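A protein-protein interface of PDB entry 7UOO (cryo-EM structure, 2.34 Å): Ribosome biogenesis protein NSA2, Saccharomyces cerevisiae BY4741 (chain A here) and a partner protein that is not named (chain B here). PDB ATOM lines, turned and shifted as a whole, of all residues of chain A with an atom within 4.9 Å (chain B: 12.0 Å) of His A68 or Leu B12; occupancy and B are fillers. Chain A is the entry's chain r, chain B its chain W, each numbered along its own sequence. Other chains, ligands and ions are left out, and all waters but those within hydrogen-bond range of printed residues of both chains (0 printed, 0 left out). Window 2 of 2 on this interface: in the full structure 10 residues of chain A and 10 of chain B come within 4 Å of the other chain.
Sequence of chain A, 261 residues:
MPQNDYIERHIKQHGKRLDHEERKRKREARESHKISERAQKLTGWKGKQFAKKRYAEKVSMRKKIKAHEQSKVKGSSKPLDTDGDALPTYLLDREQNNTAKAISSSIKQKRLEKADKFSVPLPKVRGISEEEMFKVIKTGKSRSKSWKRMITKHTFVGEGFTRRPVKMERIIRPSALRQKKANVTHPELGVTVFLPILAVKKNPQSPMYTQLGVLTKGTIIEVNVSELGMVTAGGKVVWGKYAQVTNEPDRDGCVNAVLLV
Lys A64 touches just one residue of chain B: Leu B12 (3.96 Å). Lys A66 touches none of the printed residues of chain B. No residue of chain B comes within 4 Å of Ala A67. His A68 touches two residues of chain B. No residue of chain B comes within 4 Å of Glu A69. Ser A71 touches none of the printed residues of chain B. Lys A72 touches just these residues of chain B: Ala B13 (3.5 Å) and Asp B16 (2.9 Å). Printed residues of chain A within 4 Å of Val B10: Ile A65. Leu B12 touches just these residues of chain A: Lys A64, Ile A65 and His A68. Of the printed residues of chain A, Ala B13 touches His A68 and Lys A72. Of the printed residues of chain A, Asp B16 touches Lys A72. The nearest printed residue of chain A that does not touch Leu B12 is Glu A69 (5.9 Å).
Hydrophobic or aromatic side chains of chain B that line the printed part of chain A: Val B10 and Leu B12. Of the 9 printed residues of chain A, 4 touch a printed residue of chain B. Hydrophobic or aromatic side chains of chain A within 4 Å of the printed part of chain B: Ile A65 and His A68. Along chain A the printed residues that touch a printed residue of chain B span positions 64 to 72. Among the printed residues, Asp or Glu carboxylates within 4 Å of a Lys or Arg side-chain nitrogen of the other chain: Lys A72 with Asp B16.
NE2 of His A68 sits at hydrogen-bond distance from O of Ala B13 (3.0 Å). NZ of Lys A72 is in salt-bridge range of OD1 of Asp B16 (2.9 Å).
Lys A64 touches Leu B12 (CG to CD1, 3.96 Å). Ile A65 touches Val B10 (CD1 to CG1, 3.7 Å). Ile A65 touches Leu B12 (CD1 to CD2, 3.6 Å). CD2 of His A68 touches CD2 of Leu B12 (3.6 Å). Lys A72 touches Ala B13.
The side-chain carboxylate (OE2) of Glu A69 lies within salt-bridge range of the side-chain amino group (NZ) of Lys A72 (3.5 Å).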
ATOM      1  N   LYS A  64     -29.021 -17.033   3.286  1.00  0.00           N
ATOM      2  CA  LYS A  64     -28.612 -15.884   4.092  1.00  0.00           C
ATOM      3  C   LYS A  64     -27.307 -15.280   3.578  1.00  0.00           C
ATOM      4  O   LYS A  64     -27.176 -14.051   3.491  1.00  0.00           O
ATOM      5  CB  LYS A  64     -28.478 -16.295   5.557  1.00  0.00           C
ATOM      6  CG  LYS A  64     -28.228 -15.140   6.506  1.00  0.00           C
ATOM      7  CD  LYS A  64     -28.272 -15.596   7.955  1.00  0.00           C
ATOM      8  CE  LYS A  64     -29.644 -16.142   8.318  1.00  0.00           C
ATOM      9  NZ  LYS A  64     -29.706 -16.626   9.725  1.00  0.00           N
ATOM     10  N   ILE A  65     -26.338 -16.129   3.223  1.00  0.00           N
ATOM     11  CA  ILE A  65     -25.068 -15.639   2.683  1.00  0.00           C
ATOM     12  C   ILE A  65     -25.293 -14.898   1.370  1.00  0.00           C
ATOM     13  O   ILE A  65     -24.728 -13.819   1.140  1.00  0.00           O
ATOM     14  CB  ILE A  65     -24.072 -16.800   2.501  1.00  0.00           C
ATOM     15  CG1 ILE A  65     -23.802 -17.513   3.825  1.00  0.00           C
ATOM     16  CG2 ILE A  65     -22.765 -16.295   1.912  1.00  0.00           C
ATOM     17  CD1 ILE A  65     -23.150 -16.658   4.860  1.00  0.00           C
ATOM     18  N   LYS A  66     -26.117 -15.471   0.487  1.00  0.00           N
ATOM     19  CA  LYS A  66     -26.395 -14.839  -0.800  1.00  0.00           C
ATOM     20  C   LYS A  66     -27.080 -13.490  -0.619  1.00  0.00           C
ATOM     21  O   LYS A  66     -26.727 -12.514  -1.291  1.00  0.00           O
ATOM     22  CB  LYS A  66     -27.254 -15.770  -1.658  1.00  0.00           C
ATOM     23  CG  LYS A  66     -27.793 -15.148  -2.930  1.00  0.00           C
ATOM     24  CD  LYS A  66     -26.694 -14.868  -3.938  1.00  0.00           C
ATOM     25  CE  LYS A  66     -27.269 -14.287  -5.222  1.00  0.00           C
ATOM     26  NZ  LYS A  66     -26.227 -14.055  -6.257  1.00  0.00           N
ATOM     27  N   ALA A  67     -28.051 -13.414   0.295  1.00  0.00           N
ATOM     28  CA  ALA A  67     -28.742 -12.153   0.542  1.00  0.00           C
ATOM     29  C   ALA A  67     -27.796 -11.101   1.106  1.00  0.00           C
ATOM     30  O   ALA A  67     -27.857  -9.930   0.713  1.00  0.00           O
ATOM     31  CB  ALA A  67     -29.922 -12.373   1.485  1.00  0.00           C
ATOM     32  N   HIS A  68     -26.911 -11.498   2.028  1.00  0.00           N
ATOM     33  CA  HIS A  68     -25.962 -10.539   2.587  1.00  0.00           C
ATOM     34  C   HIS A  68     -25.002 -10.019   1.526  1.00  0.00           C
ATOM     35  O   HIS A  68     -24.723  -8.815   1.471  1.00  0.00           O
ATOM     36  CB  HIS A  68     -25.179 -11.164   3.739  1.00  0.00           C
ATOM     37  CG  HIS A  68     -24.114 -10.268   4.288  1.00  0.00           C
ATOM     38  ND1 HIS A  68     -24.399  -9.154   5.046  1.00  0.00           N
ATOM     39  CD2 HIS A  68     -22.765 -10.309   4.171  1.00  0.00           C
ATOM     40  CE1 HIS A  68     -23.272  -8.552   5.382  1.00  0.00           C
ATOM     41  NE2 HIS A  68     -22.266  -9.234   4.864  1.00  0.00           N
ATOM     42  N   GLU A  69     -24.486 -10.908   0.672  1.00  0.00           N
ATOM     43  CA  GLU A  69     -23.581 -10.466  -0.385  1.00  0.00           C
ATOM     44  C   GLU A  69     -24.292  -9.550  -1.375  1.00  0.00           C
ATOM     45  O   GLU A  69     -23.728  -8.539  -1.815  1.00  0.00           O
ATOM     46  CB  GLU A  69     -22.976 -11.672  -1.102  1.00  0.00           C
ATOM     47  CG  GLU A  69     -21.963 -12.443  -0.266  1.00  0.00           C
ATOM     48  CD  GLU A  69     -20.696 -11.649  -0.002  1.00  0.00           C
ATOM     49  OE1 GLU A  69     -20.311 -10.833  -0.864  1.00  0.00           O
ATOM     50  OE2 GLU A  69     -20.084 -11.842   1.070  1.00  0.00           O
ATOM     51  N   GLN A  70     -25.539  -9.881  -1.728  1.00  0.00           N
ATOM     52  CA  GLN A  70     -26.302  -9.039  -2.643  1.00  0.00           C
ATOM     53  C   GLN A  70     -26.557  -7.661  -2.048  1.00  0.00           C
ATOM     54  O   GLN A  70     -26.475  -6.647  -2.752  1.00  0.00           O
ATOM     55  CB  GLN A  70     -27.619  -9.726  -3.004  1.00  0.00           C
ATOM     56  CG  GLN A  70     -28.493  -8.941  -3.960  1.00  0.00           C
ATOM     57  CD  GLN A  70     -29.747  -9.698  -4.358  1.00  0.00           C
ATOM     58  OE1 GLN A  70     -29.750 -10.928  -4.420  1.00  0.00           O
ATOM     59  NE2 GLN A  70     -30.820  -8.965  -4.621  1.00  0.00           N
ATOM     60  N   SER A  71     -26.869  -7.600  -0.751  1.00  0.00           N
ATOM     61  CA  SER A  71     -27.081  -6.306  -0.108  1.00  0.00           C
ATOM     62  C   SER A  71     -25.782  -5.518  -0.006  1.00  0.00           C
ATOM     63  O   SER A  71     -25.786  -4.287  -0.113  1.00  0.00           O
ATOM     64  CB  SER A  71     -27.700  -6.504   1.276  1.00  0.00           C
ATOM     65  OG  SER A  71     -27.956  -5.258   1.900  1.00  0.00           O
ATOM     66  N   LYS A  72     -24.658  -6.209   0.202  1.00  0.00           N
ATOM     67  CA  LYS A  72     -23.379  -5.521   0.342  1.00  0.00           C
ATOM     68  C   LYS A  72     -22.853  -5.020  -0.998  1.00  0.00           C
ATOM     69  O   LYS A  72     -22.060  -4.073  -1.031  1.00  0.00           O
ATOM     70  CB  LYS A  72     -22.360  -6.447   1.006  1.00  0.00           C
ATOM     71  CG  LYS A  72     -21.128  -5.746   1.552  1.00  0.00           C
ATOM     72  CD  LYS A  72     -20.292  -6.679   2.412  1.00  0.00           C
ATOM     73  CE  LYS A  72     -19.749  -7.844   1.604  1.00  0.00           C
ATOM     74  NZ  LYS A  72     -18.993  -8.807   2.451  1.00  0.00           N
ATOM     75  N   LYS B   8     -14.275 -22.977   9.417  1.00  0.00           N
ATOM     76  CA  LYS B   8     -14.050 -21.554   9.634  1.00  0.00           C
ATOM     77  C   LYS B   8     -15.359 -20.858   9.989  1.00  0.00           C
ATOM     78  O   LYS B   8     -16.390 -21.092   9.352  1.00  0.00           O
ATOM     79  CB  LYS B   8     -13.435 -20.920   8.386  1.00  0.00           C
ATOM     80  CG  LYS B   8     -12.148 -21.587   7.919  1.00  0.00           C
ATOM     81  CD  LYS B   8     -11.792 -21.177   6.496  1.00  0.00           C
ATOM     82  CE  LYS B   8     -11.452 -19.700   6.401  1.00  0.00           C
ATOM     83  NZ  LYS B   8     -10.175 -19.375   7.094  1.00  0.00           N
ATOM     84  N   LEU B   9     -15.314 -20.005  11.011  1.00  0.00           N
ATOM     85  CA  LEU B   9     -16.497 -19.257  11.417  1.00  0.00           C
ATOM     86  C   LEU B   9     -16.866 -18.222  10.362  1.00  0.00           C
ATOM     87  O   LEU B   9     -16.000 -17.549   9.797  1.00  0.00           O
ATOM     88  CB  LEU B   9     -16.259 -18.575  12.763  1.00  0.00           C
ATOM     89  CG  LEU B   9     -15.999 -19.514  13.941  1.00  0.00           C
ATOM     90  CD1 LEU B   9     -15.875 -18.738  15.244  1.00  0.00           C
ATOM     91  CD2 LEU B   9     -17.096 -20.565  14.035  1.00  0.00           C
ATOM     92  N   VAL B  10     -18.164 -18.093  10.104  1.00  0.00           N
ATOM     93  CA  VAL B  10     -18.688 -17.227   9.053  1.00  0.00           C
ATOM     94  C   VAL B  10     -19.343 -16.019   9.708  1.00  0.00           C
ATOM     95  O   VAL B  10     -20.238 -16.171  10.549  1.00  0.00           O
ATOM     96  CB  VAL B  10     -19.684 -17.973   8.152  1.00  0.00           C
ATOM     97  CG1 VAL B  10     -20.153 -17.075   7.019  1.00  0.00           C
ATOM     98  CG2 VAL B  10     -19.057 -19.248   7.611  1.00  0.00           C
ATOM     99  N   THR B  11     -18.903 -14.824   9.321  1.00  0.00           N
ATOM    100  CA  THR B  11     -19.445 -13.574   9.836  1.00  0.00           C
ATOM    101  C   THR B  11     -19.904 -12.701   8.679  1.00  0.00           C
ATOM    102  O   THR B  11     -19.247 -12.640   7.637  1.00  0.00           O
ATOM    103  CB  THR B  11     -18.412 -12.808  10.671  1.00  0.00           C
ATOM    104  OG1 THR B  11     -17.301 -12.454   9.841  1.00  0.00           O
ATOM    105  CG2 THR B  11     -17.923 -13.655  11.832  1.00  0.00           C
ATOM    106  N   LEU B  12     -21.029 -12.021   8.871  1.00  0.00           N
ATOM    107  CA  LEU B  12     -21.611 -11.137   7.863  1.00  0.00           C
ATOM    108  C   LEU B  12     -21.349  -9.697   8.291  1.00  0.00           C
ATOM    109  O   LEU B  12     -22.175  -9.073   8.960  1.00  0.00           O
ATOM    110  CB  LEU B  12     -23.102 -11.406   7.696  1.00  0.00           C
ATOM    111  CG  LEU B  12     -23.488 -12.840   7.335  1.00  0.00           C
ATOM    112  CD1 LEU B  12     -24.983 -12.946   7.104  1.00  0.00           C
ATOM    113  CD2 LEU B  12     -22.719 -13.288   6.112  1.00  0.00           C
ATOM    114  N   ALA B  13     -20.200  -9.166   7.892  1.00  0.00           N
ATOM    115  CA  ALA B  13     -19.791  -7.813   8.236  1.00  0.00           C
ATOM    116  C   ALA B  13     -19.796  -6.932   6.990  1.00  0.00           C
ATOM    117  O   ALA B  13     -20.099  -7.380   5.881  1.00  0.00           O
ATOM    118  CB  ALA B  13     -18.417  -7.824   8.905  1.00  0.00           C
ATOM    119  N   GLN B  14     -19.450  -5.659   7.185  1.00  0.00           N
ATOM    120  CA  GLN B  14     -19.499  -4.671   6.115  1.00  0.00           C
ATOM    121  C   GLN B  14     -18.142  -4.366   5.494  1.00  0.00           C
ATOM    122  O   GLN B  14     -18.099  -3.776   4.409  1.00  0.00           O
ATOM    123  CB  GLN B  14     -20.110  -3.361   6.631  1.00  0.00           C
ATOM    124  CG  GLN B  14     -21.608  -3.428   6.896  1.00  0.00           C
ATOM    125  CD  GLN B  14     -22.418  -3.553   5.622  1.00  0.00           C
ATOM    126  OE1 GLN B  14     -21.981  -3.132   4.551  1.00  0.00           O
ATOM    127  NE2 GLN B  14     -23.604  -4.137   5.730  1.00  0.00           N
ATOM    128  N   THR B  15     -17.045  -4.752   6.137  1.00  0.00           N
ATOM    129  CA  THR B  15     -15.701  -4.415   5.682  1.00  0.00           C
ATOM    130  C   THR B  15     -15.024  -5.663   5.134  1.00  0.00           C
ATOM    131  O   THR B  15     -14.932  -6.680   5.830  1.00  0.00           O
ATOM    132  CB  THR B  15     -14.876  -3.814   6.820  1.00  0.00           C
ATOM    133  OG1 THR B  15     -15.500  -2.608   7.278  1.00  0.00           O
ATOM    134  CG2 THR B  15     -13.467  -3.501   6.351  1.00  0.00           C
ATOM    135  N   ASP B  16     -14.547  -5.581   3.898  1.00  0.00           N
ATOM    136  CA  ASP B  16     -13.857  -6.681   3.243  1.00  0.00           C
ATOM    137  C   ASP B  16     -12.345  -6.507   3.352  1.00  0.00           C
ATOM    138  O   ASP B  16     -11.840  -5.434   3.688  1.00  0.00           O
ATOM    139  CB  ASP B  16     -14.276  -6.784   1.775  1.00  0.00           C
ATOM    140  CG  ASP B  16     -15.726  -7.202   1.612  1.00  0.00           C
ATOM    141  OD1 ASP B  16     -16.228  -7.959   2.471  1.00  0.00           O
ATOM    142  OD2 ASP B  16     -16.365  -6.777   0.627  1.00  0.00           O
ATOM    143  N   LYS B  17     -11.626  -7.590   3.066  1.00  0.00           N
ATOM    144  CA  LYS B  17     -10.177  -7.596   3.218  1.00  0.00           C
ATOM    145  C   LYS B  17      -9.497  -6.787   2.121  1.00  0.00           C
ATOM    146  O   LYS B  17     -10.017  -6.629   1.014  1.00  0.00           O
ATOM    147  CB  LYS B  17      -9.644  -9.029   3.207  1.00  0.00           C
ATOM    148  CG  LYS B  17      -9.647  -9.704   4.568  1.00  0.00           C
ATOM    149  CD  LYS B  17      -9.231 -11.163   4.469  1.00  0.00           C
ATOM    150  CE  LYS B  17      -9.296 -11.846   5.826  1.00  0.00           C
ATOM    151  NZ  LYS B  17      -8.941 -13.288   5.749  1.00  0.00           N
